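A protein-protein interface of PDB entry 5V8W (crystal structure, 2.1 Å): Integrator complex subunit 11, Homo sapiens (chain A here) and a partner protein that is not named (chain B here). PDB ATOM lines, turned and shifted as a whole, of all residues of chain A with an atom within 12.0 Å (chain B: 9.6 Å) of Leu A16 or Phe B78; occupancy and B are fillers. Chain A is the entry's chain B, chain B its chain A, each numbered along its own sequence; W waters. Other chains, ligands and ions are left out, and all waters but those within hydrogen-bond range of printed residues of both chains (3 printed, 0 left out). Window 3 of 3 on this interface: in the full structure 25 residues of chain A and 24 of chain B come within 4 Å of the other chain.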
ATOM      1  N   VAL A   7       3.490  12.763  14.408  1.00  0.00           N
ATOM      2  CA  VAL A   7       3.129  11.695  13.480  1.00  0.00           C
ATOM      3  C   VAL A   7       3.202  12.229  12.043  1.00  0.00           C
ATOM      4  O   VAL A   7       2.988  13.420  11.822  1.00  0.00           O
ATOM      5  CB  VAL A   7       1.706  11.117  13.813  1.00  0.00           C
ATOM      6  CG1 VAL A   7       0.584  12.121  13.493  1.00  0.00           C
ATOM      7  CG2 VAL A   7       1.466   9.788  13.111  1.00  0.00           C
ATOM      8  N   SER A   8       3.532  11.369  11.075  1.00  0.00           N
ATOM      9  CA  SER A   8       3.535  11.764   9.656  1.00  0.00           C
ATOM     10  C   SER A   8       2.147  11.586   9.016  1.00  0.00           C
ATOM     11  O   SER A   8       1.196  11.202   9.704  1.00  0.00           O
ATOM     12  CB  SER A   8       4.578  10.965   8.870  1.00  0.00           C
ATOM     13  OG  SER A   8       4.104   9.668   8.555  1.00  0.00           O
ATOM     14  N   SER A   9       2.031  11.850   7.709  1.00  0.00           N
ATOM     15  CA  SER A   9       0.727  11.771   7.025  1.00  0.00           C
ATOM     16  C   SER A   9       0.287  10.339   6.685  1.00  0.00           C
ATOM     17  O   SER A   9      -0.913  10.041   6.721  1.00  0.00           O
ATOM     18  CB  SER A   9       0.726  12.612   5.736  1.00  0.00           C
ATOM     19  OG  SER A   9       0.322  13.952   5.977  1.00  0.00           O
ATOM     20  N   GLU A  10       1.238   9.463   6.351  1.00  0.00           N
ATOM     21  CA  GLU A  10       0.908   8.066   6.050  1.00  0.00           C
ATOM     22  C   GLU A  10       0.716   7.253   7.328  1.00  0.00           C
ATOM     23  O   GLU A  10      -0.120   6.351   7.366  1.00  0.00           O
ATOM     24  CB  GLU A  10       1.979   7.409   5.173  1.00  0.00           C
ATOM     25  CG  GLU A  10       1.964   7.862   3.721  1.00  0.00           C
ATOM     26  CD  GLU A  10       3.011   8.921   3.442  1.00  0.00           C
ATOM     27  OE1 GLU A  10       4.118   8.819   4.017  1.00  0.00           O
ATOM     28  OE2 GLU A  10       2.733   9.854   2.653  1.00  0.00           O
ATOM     29  N   GLN A  11       1.487   7.567   8.367  1.00  0.00           N
ATOM     30  CA  GLN A  11       1.297   6.933   9.671  1.00  0.00           C
ATOM     31  C   GLN A  11      -0.073   7.309  10.249  1.00  0.00           C
ATOM     32  O   GLN A  11      -0.739   6.475  10.864  1.00  0.00           O
ATOM     33  CB  GLN A  11       2.407   7.327  10.656  1.00  0.00           C
ATOM     34  CG  GLN A  11       3.770   6.731  10.377  1.00  0.00           C
ATOM     35  CD  GLN A  11       4.857   7.381  11.215  1.00  0.00           C
ATOM     36  OE1 GLN A  11       4.636   8.420  11.838  1.00  0.00           O
ATOM     37  NE2 GLN A  11       6.038   6.769  11.235  1.00  0.00           N
ATOM     38  N   ALA A  12      -0.494   8.559  10.050  1.00  0.00           N
ATOM     39  CA  ALA A  12      -1.775   9.034  10.575  1.00  0.00           C
ATOM     40  C   ALA A  12      -2.950   8.450   9.792  1.00  0.00           C
ATOM     41  O   ALA A  12      -4.076   8.403  10.299  1.00  0.00           O
ATOM     42  CB  ALA A  12      -1.832  10.551  10.561  1.00  0.00           C
ATOM     43  N   LEU A  13      -2.682   8.010   8.562  1.00  0.00           N
ATOM     44  CA  LEU A  13      -3.669   7.278   7.773  1.00  0.00           C
ATOM     45  C   LEU A  13      -3.739   5.824   8.241  1.00  0.00           C
ATOM     46  O   LEU A  13      -4.820   5.309   8.539  1.00  0.00           O
ATOM     47  CB  LEU A  13      -3.341   7.342   6.270  1.00  0.00           C
ATOM     48  CG  LEU A  13      -4.140   8.312   5.398  1.00  0.00           C
ATOM     49  CD1 LEU A  13      -3.604   8.330   3.992  1.00  0.00           C
ATOM     50  CD2 LEU A  13      -5.587   7.914   5.398  1.00  0.00           C
ATOM     51  N   LYS A  14      -2.582   5.171   8.303  1.00  0.00           N
ATOM     52  CA  LYS A  14      -2.500   3.760   8.700  1.00  0.00           C
ATOM     53  C   LYS A  14      -2.997   3.503  10.134  1.00  0.00           C
ATOM     54  O   LYS A  14      -3.576   2.449  10.403  1.00  0.00           O
ATOM     55  CB  LYS A  14      -1.061   3.245   8.538  1.00  0.00           C
ATOM     56  CG  LYS A  14      -0.580   3.183   7.074  1.00  0.00           C
ATOM     57  CD  LYS A  14       0.885   2.734   6.960  1.00  0.00           C
ATOM     58  CE  LYS A  14       1.406   2.868   5.527  1.00  0.00           C
ATOM     59  NZ  LYS A  14       2.811   3.367   5.488  1.00  0.00           N
ATOM     60  N   GLU A  15      -2.790   4.469  11.036  1.00  0.00           N
ATOM     61  CA  GLU A  15      -3.226   4.369  12.446  1.00  0.00           C
ATOM     62  C   GLU A  15      -4.757   4.405  12.607  1.00  0.00           C
ATOM     63  O   GLU A  15      -5.278   4.078  13.674  1.00  0.00           O
ATOM     64  CB  GLU A  15      -2.594   5.496  13.297  1.00  0.00           C
ATOM     65  CG  GLU A  15      -1.169   5.211  13.832  1.00  0.00           C
ATOM     66  CD  GLU A  15      -0.571   6.358  14.677  1.00  0.00           C
ATOM     67  OE1 GLU A  15      -1.186   7.447  14.751  1.00  0.00           O
ATOM     68  OE2 GLU A  15       0.521   6.171  15.264  1.00  0.00           O
ATOM     69  N   LEU A  16      -5.467   4.806  11.552  1.00  0.00           N
ATOM     70  CA  LEU A  16      -6.931   4.894  11.575  1.00  0.00           C
ATOM     71  C   LEU A  16      -7.580   3.840  10.677  1.00  0.00           C
ATOM     72  O   LEU A  16      -8.803   3.850  10.475  1.00  0.00           O
ATOM     73  CB  LEU A  16      -7.392   6.295  11.150  1.00  0.00           C
ATOM     74  CG  LEU A  16      -7.203   7.413  12.176  1.00  0.00           C
ATOM     75  CD1 LEU A  16      -7.474   8.771  11.559  1.00  0.00           C
ATOM     76  CD2 LEU A  16      -8.102   7.173  13.394  1.00  0.00           C
ATOM     77  N   GLY A  17      -6.758   2.933  10.153  1.00  0.00           N
ATOM     78  CA  GLY A  17      -7.218   1.920   9.219  1.00  0.00           C
ATOM     79  C   GLY A  17      -7.645   2.418   7.837  1.00  0.00           C
ATOM     80  O   GLY A  17      -8.184   1.644   7.042  1.00  0.00           O
ATOM     81  N   LEU A  18      -7.400   3.690   7.527  1.00  0.00           N
ATOM     82  CA  LEU A  18      -7.910   4.275   6.273  1.00  0.00           C
ATOM     83  C   LEU A  18      -6.985   4.082   5.065  1.00  0.00           C
ATOM     84  O   LEU A  18      -5.764   3.994   5.212  1.00  0.00           O
ATOM     85  CB  LEU A  18      -8.177   5.768   6.465  1.00  0.00           C
ATOM     86  CG  LEU A  18      -8.912   6.115   7.757  1.00  0.00           C
ATOM     87  CD1 LEU A  18      -8.855   7.611   8.029  1.00  0.00           C
ATOM     88  CD2 LEU A  18     -10.346   5.611   7.687  1.00  0.00           C
ATOM     89  N   ALA A  19      -7.587   4.010   3.875  1.00  0.00           N
ATOM     90  CA  ALA A  19      -6.854   3.948   2.621  1.00  0.00           C
ATOM     91  C   ALA A  19      -6.739   5.341   2.053  1.00  0.00           C
ATOM     92  O   ALA A  19      -7.558   6.214   2.345  1.00  0.00           O
ATOM     93  CB  ALA A  19      -7.544   3.039   1.618  1.00  0.00           C
ATOM     94  N   GLU A  20      -5.720   5.565   1.244  1.00  0.00           N
ATOM     95  CA  GLU A  20      -5.595   6.852   0.609  1.00  0.00           C
ATOM     96  C   GLU A  20      -6.650   6.965  -0.498  1.00  0.00           C
ATOM     97  O   GLU A  20      -6.943   5.982  -1.180  1.00  0.00           O
ATOM     98  CB  GLU A  20      -4.186   7.053   0.050  1.00  0.00           C
ATOM     99  CG  GLU A  20      -3.991   8.423  -0.564  1.00  0.00           C
ATOM    100  CD  GLU A  20      -2.604   8.632  -1.174  1.00  0.00           C
ATOM    101  OE1 GLU A  20      -2.431   9.684  -1.818  1.00  0.00           O
ATOM    102  OE2 GLU A  20      -1.700   7.772  -1.015  1.00  0.00           O
ATOM    103  N   HIS A  21      -7.221   8.163  -0.647  1.00  0.00           N
ATOM    104  CA  HIS A  21      -8.140   8.482  -1.740  1.00  0.00           C
ATOM    105  C   HIS A  21      -7.326   9.147  -2.826  1.00  0.00           C
ATOM    106  O   HIS A  21      -6.700  10.183  -2.560  1.00  0.00           O
ATOM    107  CB  HIS A  21      -9.268   9.420  -1.271  1.00  0.00           C
ATOM    108  CG  HIS A  21     -10.422   9.532  -2.232  1.00  0.00           C
ATOM    109  ND1 HIS A  21     -11.616   8.863  -2.041  1.00  0.00           N
ATOM    110  CD2 HIS A  21     -10.572  10.252  -3.374  1.00  0.00           C
ATOM    111  CE1 HIS A  21     -12.444   9.148  -3.037  1.00  0.00           C
ATOM    112  NE2 HIS A  21     -11.837   9.990  -3.860  1.00  0.00           N
ATOM    113  N   GLN A  22      -7.323   8.569  -4.033  1.00  0.00           N
ATOM    114  CA  GLN A  22      -6.627   9.189  -5.166  1.00  0.00           C
ATOM    115  C   GLN A  22      -7.575  10.156  -5.855  1.00  0.00           C
ATOM    116  O   GLN A  22      -8.622   9.750  -6.356  1.00  0.00           O
ATOM    117  CB  GLN A  22      -6.107   8.134  -6.168  1.00  0.00           C
ATOM    118  CG  GLN A  22      -5.352   8.756  -7.392  1.00  0.00           C
ATOM    119  CD  GLN A  22      -5.134   7.802  -8.620  1.00  0.00           C
ATOM    120  OE1 GLN A  22      -6.085   7.365  -9.276  1.00  0.00           O
ATOM    121  NE2 GLN A  22      -3.870   7.536  -8.944  1.00  0.00           N
ATOM    122  N   LEU A  23      -7.224  11.444  -5.852  1.00  0.00           N
ATOM    123  CA  LEU A  23      -7.960  12.421  -6.647  1.00  0.00           C
ATOM    124  C   LEU A  23      -7.166  12.764  -7.900  1.00  0.00           C
ATOM    125  O   LEU A  23      -6.075  13.334  -7.830  1.00  0.00           O
ATOM    126  CB  LEU A  23      -8.250  13.690  -5.850  1.00  0.00           C
ATOM    127  CG  LEU A  23      -8.865  14.885  -6.601  1.00  0.00           C
ATOM    128  CD1 LEU A  23     -10.206  14.581  -7.268  1.00  0.00           C
ATOM    129  CD2 LEU A  23      -9.020  16.081  -5.640  1.00  0.00           C
ATOM    130  N   TYR A  92      -3.820  14.966  -7.211  1.00  0.00           N
ATOM    131  CA  TYR A  92      -3.900  16.116  -6.339  1.00  0.00           C
ATOM    132  C   TYR A  92      -2.534  16.492  -5.723  1.00  0.00           C
ATOM    133  O   TYR A  92      -2.264  17.678  -5.558  1.00  0.00           O
ATOM    134  CB  TYR A  92      -4.952  15.870  -5.244  1.00  0.00           C
ATOM    135  CG  TYR A  92      -5.227  17.124  -4.462  1.00  0.00           C
ATOM    136  CD1 TYR A  92      -5.710  18.258  -5.109  1.00  0.00           C
ATOM    137  CD2 TYR A  92      -4.964  17.201  -3.097  1.00  0.00           C
ATOM    138  CE1 TYR A  92      -5.945  19.430  -4.420  1.00  0.00           C
ATOM    139  CE2 TYR A  92      -5.204  18.377  -2.388  1.00  0.00           C
ATOM    140  CZ  TYR A  92      -5.694  19.490  -3.060  1.00  0.00           C
ATOM    141  OH  TYR A  92      -5.939  20.671  -2.408  1.00  0.00           O
ATOM    142  N   GLN A  93      -1.674  15.507  -5.433  1.00  0.00           N
ATOM    143  CA  GLN A  93      -0.285  15.765  -5.011  1.00  0.00           C
ATOM    144  C   GLN A  93       0.440  16.783  -5.895  1.00  0.00           C
ATOM    145  O   GLN A  93       1.260  17.588  -5.413  1.00  0.00           O
ATOM    146  CB  GLN A  93       0.559  14.476  -5.013  1.00  0.00           C
ATOM    147  CG  GLN A  93       0.176  13.454  -3.981  1.00  0.00           C
ATOM    148  CD  GLN A  93      -0.220  14.082  -2.661  1.00  0.00           C
ATOM    149  OE1 GLN A  93      -1.410  14.120  -2.305  1.00  0.00           O
ATOM    150  NE2 GLN A  93       0.776  14.589  -1.922  1.00  0.00           N
ATOM    151  N   LYS B   2       0.903  19.427  -0.917  1.00  0.00           N
ATOM    152  CA  LYS B   2      -0.501  19.072  -0.715  1.00  0.00           C
ATOM    153  C   LYS B   2      -0.674  17.904   0.281  1.00  0.00           C
ATOM    154  O   LYS B   2       0.215  17.058   0.437  1.00  0.00           O
ATOM    155  CB  LYS B   2      -1.171  18.732  -2.066  1.00  0.00           C
ATOM    156  CG  LYS B   2      -1.418  19.941  -3.001  1.00  0.00           C
ATOM    157  CD  LYS B   2      -2.425  20.923  -2.400  1.00  0.00           C
ATOM    158  CE  LYS B   2      -2.766  22.074  -3.352  1.00  0.00           C
ATOM    159  NZ  LYS B   2      -1.672  23.077  -3.506  1.00  0.00           N
ATOM    160  N   PRO B   3      -1.828  17.863   0.972  1.00  0.00           N
ATOM    161  CA  PRO B   3      -2.089  16.777   1.925  1.00  0.00           C
ATOM    162  C   PRO B   3      -2.574  15.484   1.264  1.00  0.00           C
ATOM    163  O   PRO B   3      -3.202  15.524   0.201  1.00  0.00           O
ATOM    164  CB  PRO B   3      -3.195  17.363   2.821  1.00  0.00           C
ATOM    165  CG  PRO B   3      -3.947  18.280   1.919  1.00  0.00           C
ATOM    166  CD  PRO B   3      -2.894  18.886   1.001  1.00  0.00           C
ATOM    167  N   LEU B   4      -2.288  14.354   1.904  1.00  0.00           N
ATOM    168  CA  LEU B   4      -2.959  13.108   1.571  1.00  0.00           C
ATOM    169  C   LEU B   4      -4.461  13.240   1.855  1.00  0.00           C
ATOM    170  O   LEU B   4      -4.859  13.972   2.751  1.00  0.00           O
ATOM    171  CB  LEU B   4      -2.362  11.937   2.355  1.00  0.00           C
ATOM    172  CG  LEU B   4      -0.862  11.709   2.146  1.00  0.00           C
ATOM    173  CD1 LEU B   4      -0.475  10.365   2.695  1.00  0.00           C
ATOM    174  CD2 LEU B   4      -0.441  11.834   0.674  1.00  0.00           C
ATOM    175  N   LEU B   5      -5.272  12.535   1.067  1.00  0.00           N
ATOM    176  CA  LEU B   5      -6.736  12.563   1.142  1.00  0.00           C
ATOM    177  C   LEU B   5      -7.249  11.177   1.492  1.00  0.00           C
ATOM    178  O   LEU B   5      -6.627  10.182   1.136  1.00  0.00           O
ATOM    179  CB  LEU B   5      -7.352  13.008  -0.202  1.00  0.00           C
ATOM    180  CG  LEU B   5      -6.907  14.359  -0.747  1.00  0.00           C
ATOM    181  CD1 LEU B   5      -7.393  14.558  -2.195  1.00  0.00           C
ATOM    182  CD2 LEU B   5      -7.444  15.479   0.178  1.00  0.00           C
ATOM    183  N   SER B   6      -8.365  11.098   2.205  1.00  0.00           N
ATOM    184  CA  SER B   6      -9.082   9.826   2.331  1.00  0.00           C
ATOM    185  C   SER B   6     -10.571  10.087   2.516  1.00  0.00           C
ATOM    186  O   SER B   6     -10.993  11.197   2.846  1.00  0.00           O
ATOM    187  CB  SER B   6      -8.545   8.980   3.487  1.00  0.00           C
ATOM    188  OG  SER B   6      -8.964   9.488   4.719  1.00  0.00           O
ATOM    189  N   GLY B   7     -11.363   9.056   2.290  1.00  0.00           N
ATOM    190  CA  GLY B   7     -12.790   9.155   2.476  1.00  0.00           C
ATOM    191  C   GLY B   7     -13.528   8.792   1.206  1.00  0.00           C
ATOM    192  O   GLY B   7     -12.946   8.280   0.254  1.00  0.00           O
ATOM    193  N   LEU B  72     -13.126  18.004  -2.708  1.00  0.00           N
ATOM    194  CA  LEU B  72     -12.285  18.104  -1.506  1.00  0.00           C
ATOM    195  C   LEU B  72     -13.094  18.292  -0.212  1.00  0.00           C
ATOM    196  O   LEU B  72     -12.674  17.816   0.846  1.00  0.00           O
ATOM    197  CB  LEU B  72     -11.271  19.248  -1.649  1.00  0.00           C
ATOM    198  CG  LEU B  72     -10.142  18.966  -2.660  1.00  0.00           C
ATOM    199  CD1 LEU B  72      -9.296  20.233  -2.940  1.00  0.00           C
ATOM    200  CD2 LEU B  72      -9.259  17.805  -2.163  1.00  0.00           C
ATOM    201  N   LEU B  75     -13.817  15.051   1.464  1.00  0.00           N
ATOM    202  CA  LEU B  75     -12.686  14.236   1.890  1.00  0.00           C
ATOM    203  C   LEU B  75     -11.975  14.801   3.129  1.00  0.00           C
ATOM    204  O   LEU B  75     -12.029  16.001   3.396  1.00  0.00           O
ATOM    205  CB  LEU B  75     -11.713  14.099   0.709  1.00  0.00           C
ATOM    206  CG  LEU B  75     -12.498  13.472  -0.464  1.00  0.00           C
ATOM    207  CD1 LEU B  75     -11.755  13.570  -1.792  1.00  0.00           C
ATOM    208  CD2 LEU B  75     -12.826  11.997  -0.142  1.00  0.00           C
ATOM    209  N   GLN B  76     -11.326  13.921   3.885  1.00  0.00           N
ATOM    210  CA  GLN B  76     -10.438  14.323   4.984  1.00  0.00           C
ATOM    211  C   GLN B  76      -8.982  14.568   4.502  1.00  0.00           C
ATOM    212  O   GLN B  76      -8.476  13.853   3.627  1.00  0.00           O
ATOM    213  CB  GLN B  76     -10.457  13.262   6.094  1.00  0.00           C
ATOM    214  CG  GLN B  76     -11.856  13.024   6.742  1.00  0.00           C
ATOM    215  CD  GLN B  76     -12.719  11.998   5.980  1.00  0.00           C
ATOM    216  OE1 GLN B  76     -13.689  12.361   5.290  1.00  0.00           O
ATOM    217  NE2 GLN B  76     -12.369  10.713   6.107  1.00  0.00           N
ATOM    218  N   LYS B  77      -8.322  15.579   5.077  1.00  0.00           N
ATOM    219  CA  LYS B  77      -6.976  15.983   4.644  1.00  0.00           C
ATOM    220  C   LYS B  77      -5.903  15.611   5.658  1.00  0.00           C
ATOM    221  O   LYS B  77      -5.919  16.114   6.778  1.00  0.00           O
ATOM    222  CB  LYS B  77      -6.918  17.496   4.396  1.00  0.00           C
ATOM    223  CG  LYS B  77      -8.272  18.107   4.022  1.00  0.00           C
ATOM    224  CD  LYS B  77      -8.342  18.507   2.558  1.00  0.00           C
ATOM    225  CE  LYS B  77      -9.747  18.281   2.002  1.00  0.00           C
ATOM    226  NZ  LYS B  77     -10.819  18.498   3.023  1.00  0.00           N
ATOM    227  N   PHE B  78      -4.953  14.761   5.262  1.00  0.00           N
ATOM    228  CA  PHE B  78      -3.854  14.374   6.159  1.00  0.00           C
ATOM    229  C   PHE B  78      -2.494  14.936   5.717  1.00  0.00           C
ATOM    230  O   PHE B  78      -1.825  15.664   6.470  1.00  0.00           O
ATOM    231  CB  PHE B  78      -3.785  12.846   6.282  1.00  0.00           C
ATOM    232  CG  PHE B  78      -4.973  12.246   6.992  1.00  0.00           C
ATOM    233  CD1 PHE B  78      -6.157  11.994   6.305  1.00  0.00           C
ATOM    234  CD2 PHE B  78      -4.913  11.951   8.355  1.00  0.00           C
ATOM    235  CE1 PHE B  78      -7.253  11.449   6.961  1.00  0.00           C
ATOM    236  CE2 PHE B  78      -6.006  11.404   9.018  1.00  0.00           C
ATOM    237  CZ  PHE B  78      -7.180  11.155   8.318  1.00  0.00           C
HETATM  238  O   HOH W   1       2.434  17.640  -3.108  1.00  0.00           O
HETATM  239  O   HOH W   2      -4.566  11.536  -1.626  1.00  0.00           O
HETATM  240  O   HOH W   3       0.142  16.858   4.451  1.00  0.00           O
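The backbone NH of His A21 sits at hydrogen-bond distance from the backbone carbonyl oxygen of Leu B5.
O of Lys B2 sits at hydrogen-bond distance from NE2 of Gln A93.
The backbone carbonyl oxygen (O) of Phe B78 lies within hydrogen-bond range of the side-chain hydroxyl (OG) of Ser A9.
A ring nitrogen (ND1) of His A21 sits at hydrogen-bond distance from the backbone carbonyl oxygen (O) of Gly B7, at 2.7 Å.
O of Pro B3 lies close to OE1 of Gln A93 (3.4 Å).
The side-chain amino group of Lys B77 sits at hydrogen-bond distance from the backbone carbonyl oxygen of Leu B72, 2.9 Å away.
The backbone carbonyl oxygen (O) of Ser B6 is in hydrogen-bond range of the backbone NH (N) of Gln B76.
N of Tyr A92 lies within hydrogen-bond range of O of Leu A23 (2.9 Å).
N of Leu A18 sits at hydrogen-bond distance from O of Leu A13, at 3.2 Å.
O of Leu B4 lies within hydrogen-bond range of N of Phe B78, at 2.6 Å.
O of Leu B75 is in hydrogen-bond range of NZ of Lys B77 (2.8 Å).
Among the printed residues, merely in contact across the chains: Ser A9 with Leu B4 (3.97 Å), Glu A10 with Leu B4 (3.2 Å), Ala A12 with Phe B78 (3.8 Å), Leu A13 with Leu B4 (3.95 Å), Leu A13 with Ser B6 (3.7 Å), Leu A16 with Phe B78 (3.9 Å), Leu A18 with Ser B6 (3.8 Å), Leu A18 with Phe B78 (3.9 Å), Ala A19 with Ser B6 (3.2 Å), Glu A20 with Leu B4 (3.8 Å), Glu A20 with Leu B5 (3.5 Å), His A21 with Ser B6 (3.6 Å), His A21 with Leu B75 (3.9 Å), Leu A23 with Leu B5 (3.9 Å), Leu A23 with Leu B72 (3.9 Å), Tyr A92 with Lys B2 (3.5 Å), Tyr A92 with Leu B5 (3.7 Å), Tyr A92 with Leu B72 (3.4 Å) and Gln A93 with Leu B4 (3.9 Å).
Of the printed residues of chain B, Glu A10 touches Leu B4.
Printed residues of chain B within 4 Å of Leu A13: Leu B4 (3.95 Å) and Ser B6 (3.7 Å).
Of chain B, only Phe B78 comes within 4 Å of Leu A16.
No residue of chain B comes within 4 Å of Gly A17.
Printed residues of chain B within 4 Å of Glu A20: Leu B4 and Leu B5.
Pro B3 touches just one residue of chain A: Gln A93 (3.4 Å).
Of chain A, only Ser A9, Glu A10, Leu A13, Glu A20 and Gln A93 come within 4 Å of Leu B4.
Leu B5 touches just these residues of chain A: Glu A20 (3.5 Å), His A21 (2.8 Å), Leu A23 (3.9 Å) and Tyr A92 (3.7 Å).
Ser B6 touches four residues of chain A.
Of the printed residues of chain A, Leu B72 touches Leu A23 (3.9 Å) and Tyr A92 (3.4 Å).
No residue of chain A comes within 4 Å of Gln B76.
Phe B78 touches just these residues of chain A: Ser A9, Ala A12, Leu A16 and Leu A18.
The nearest residue of chain B that does not touch Leu A16 is Ser B6 (7.0 Å).
The nearest printed residue of chain A that does not touch Lys B2 is Ser A9 (6.4 Å).
Hydrophobic or aromatic side chains of chain A that line the printed part of chain B: Leu A13, Leu A16, Leu A18, His A21, Leu A23 and Tyr A92.
Among the printed residues, 24 pairs touch across the chains.
Water W1 lies within hydrogen-bond range of the backbone carbonyl oxygen of Gln A93 (2.6 Å) and the backbone NH of Lys B2 (3.2 Å).
Water W2 lies within hydrogen-bond range of the backbone carbonyl oxygen of His A21, the side-chain carboxylate of Glu A20 and the backbone NH of Leu B5.
Water W3 lies within hydrogen-bond range of O of Phe B78 and OG of Ser A9.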
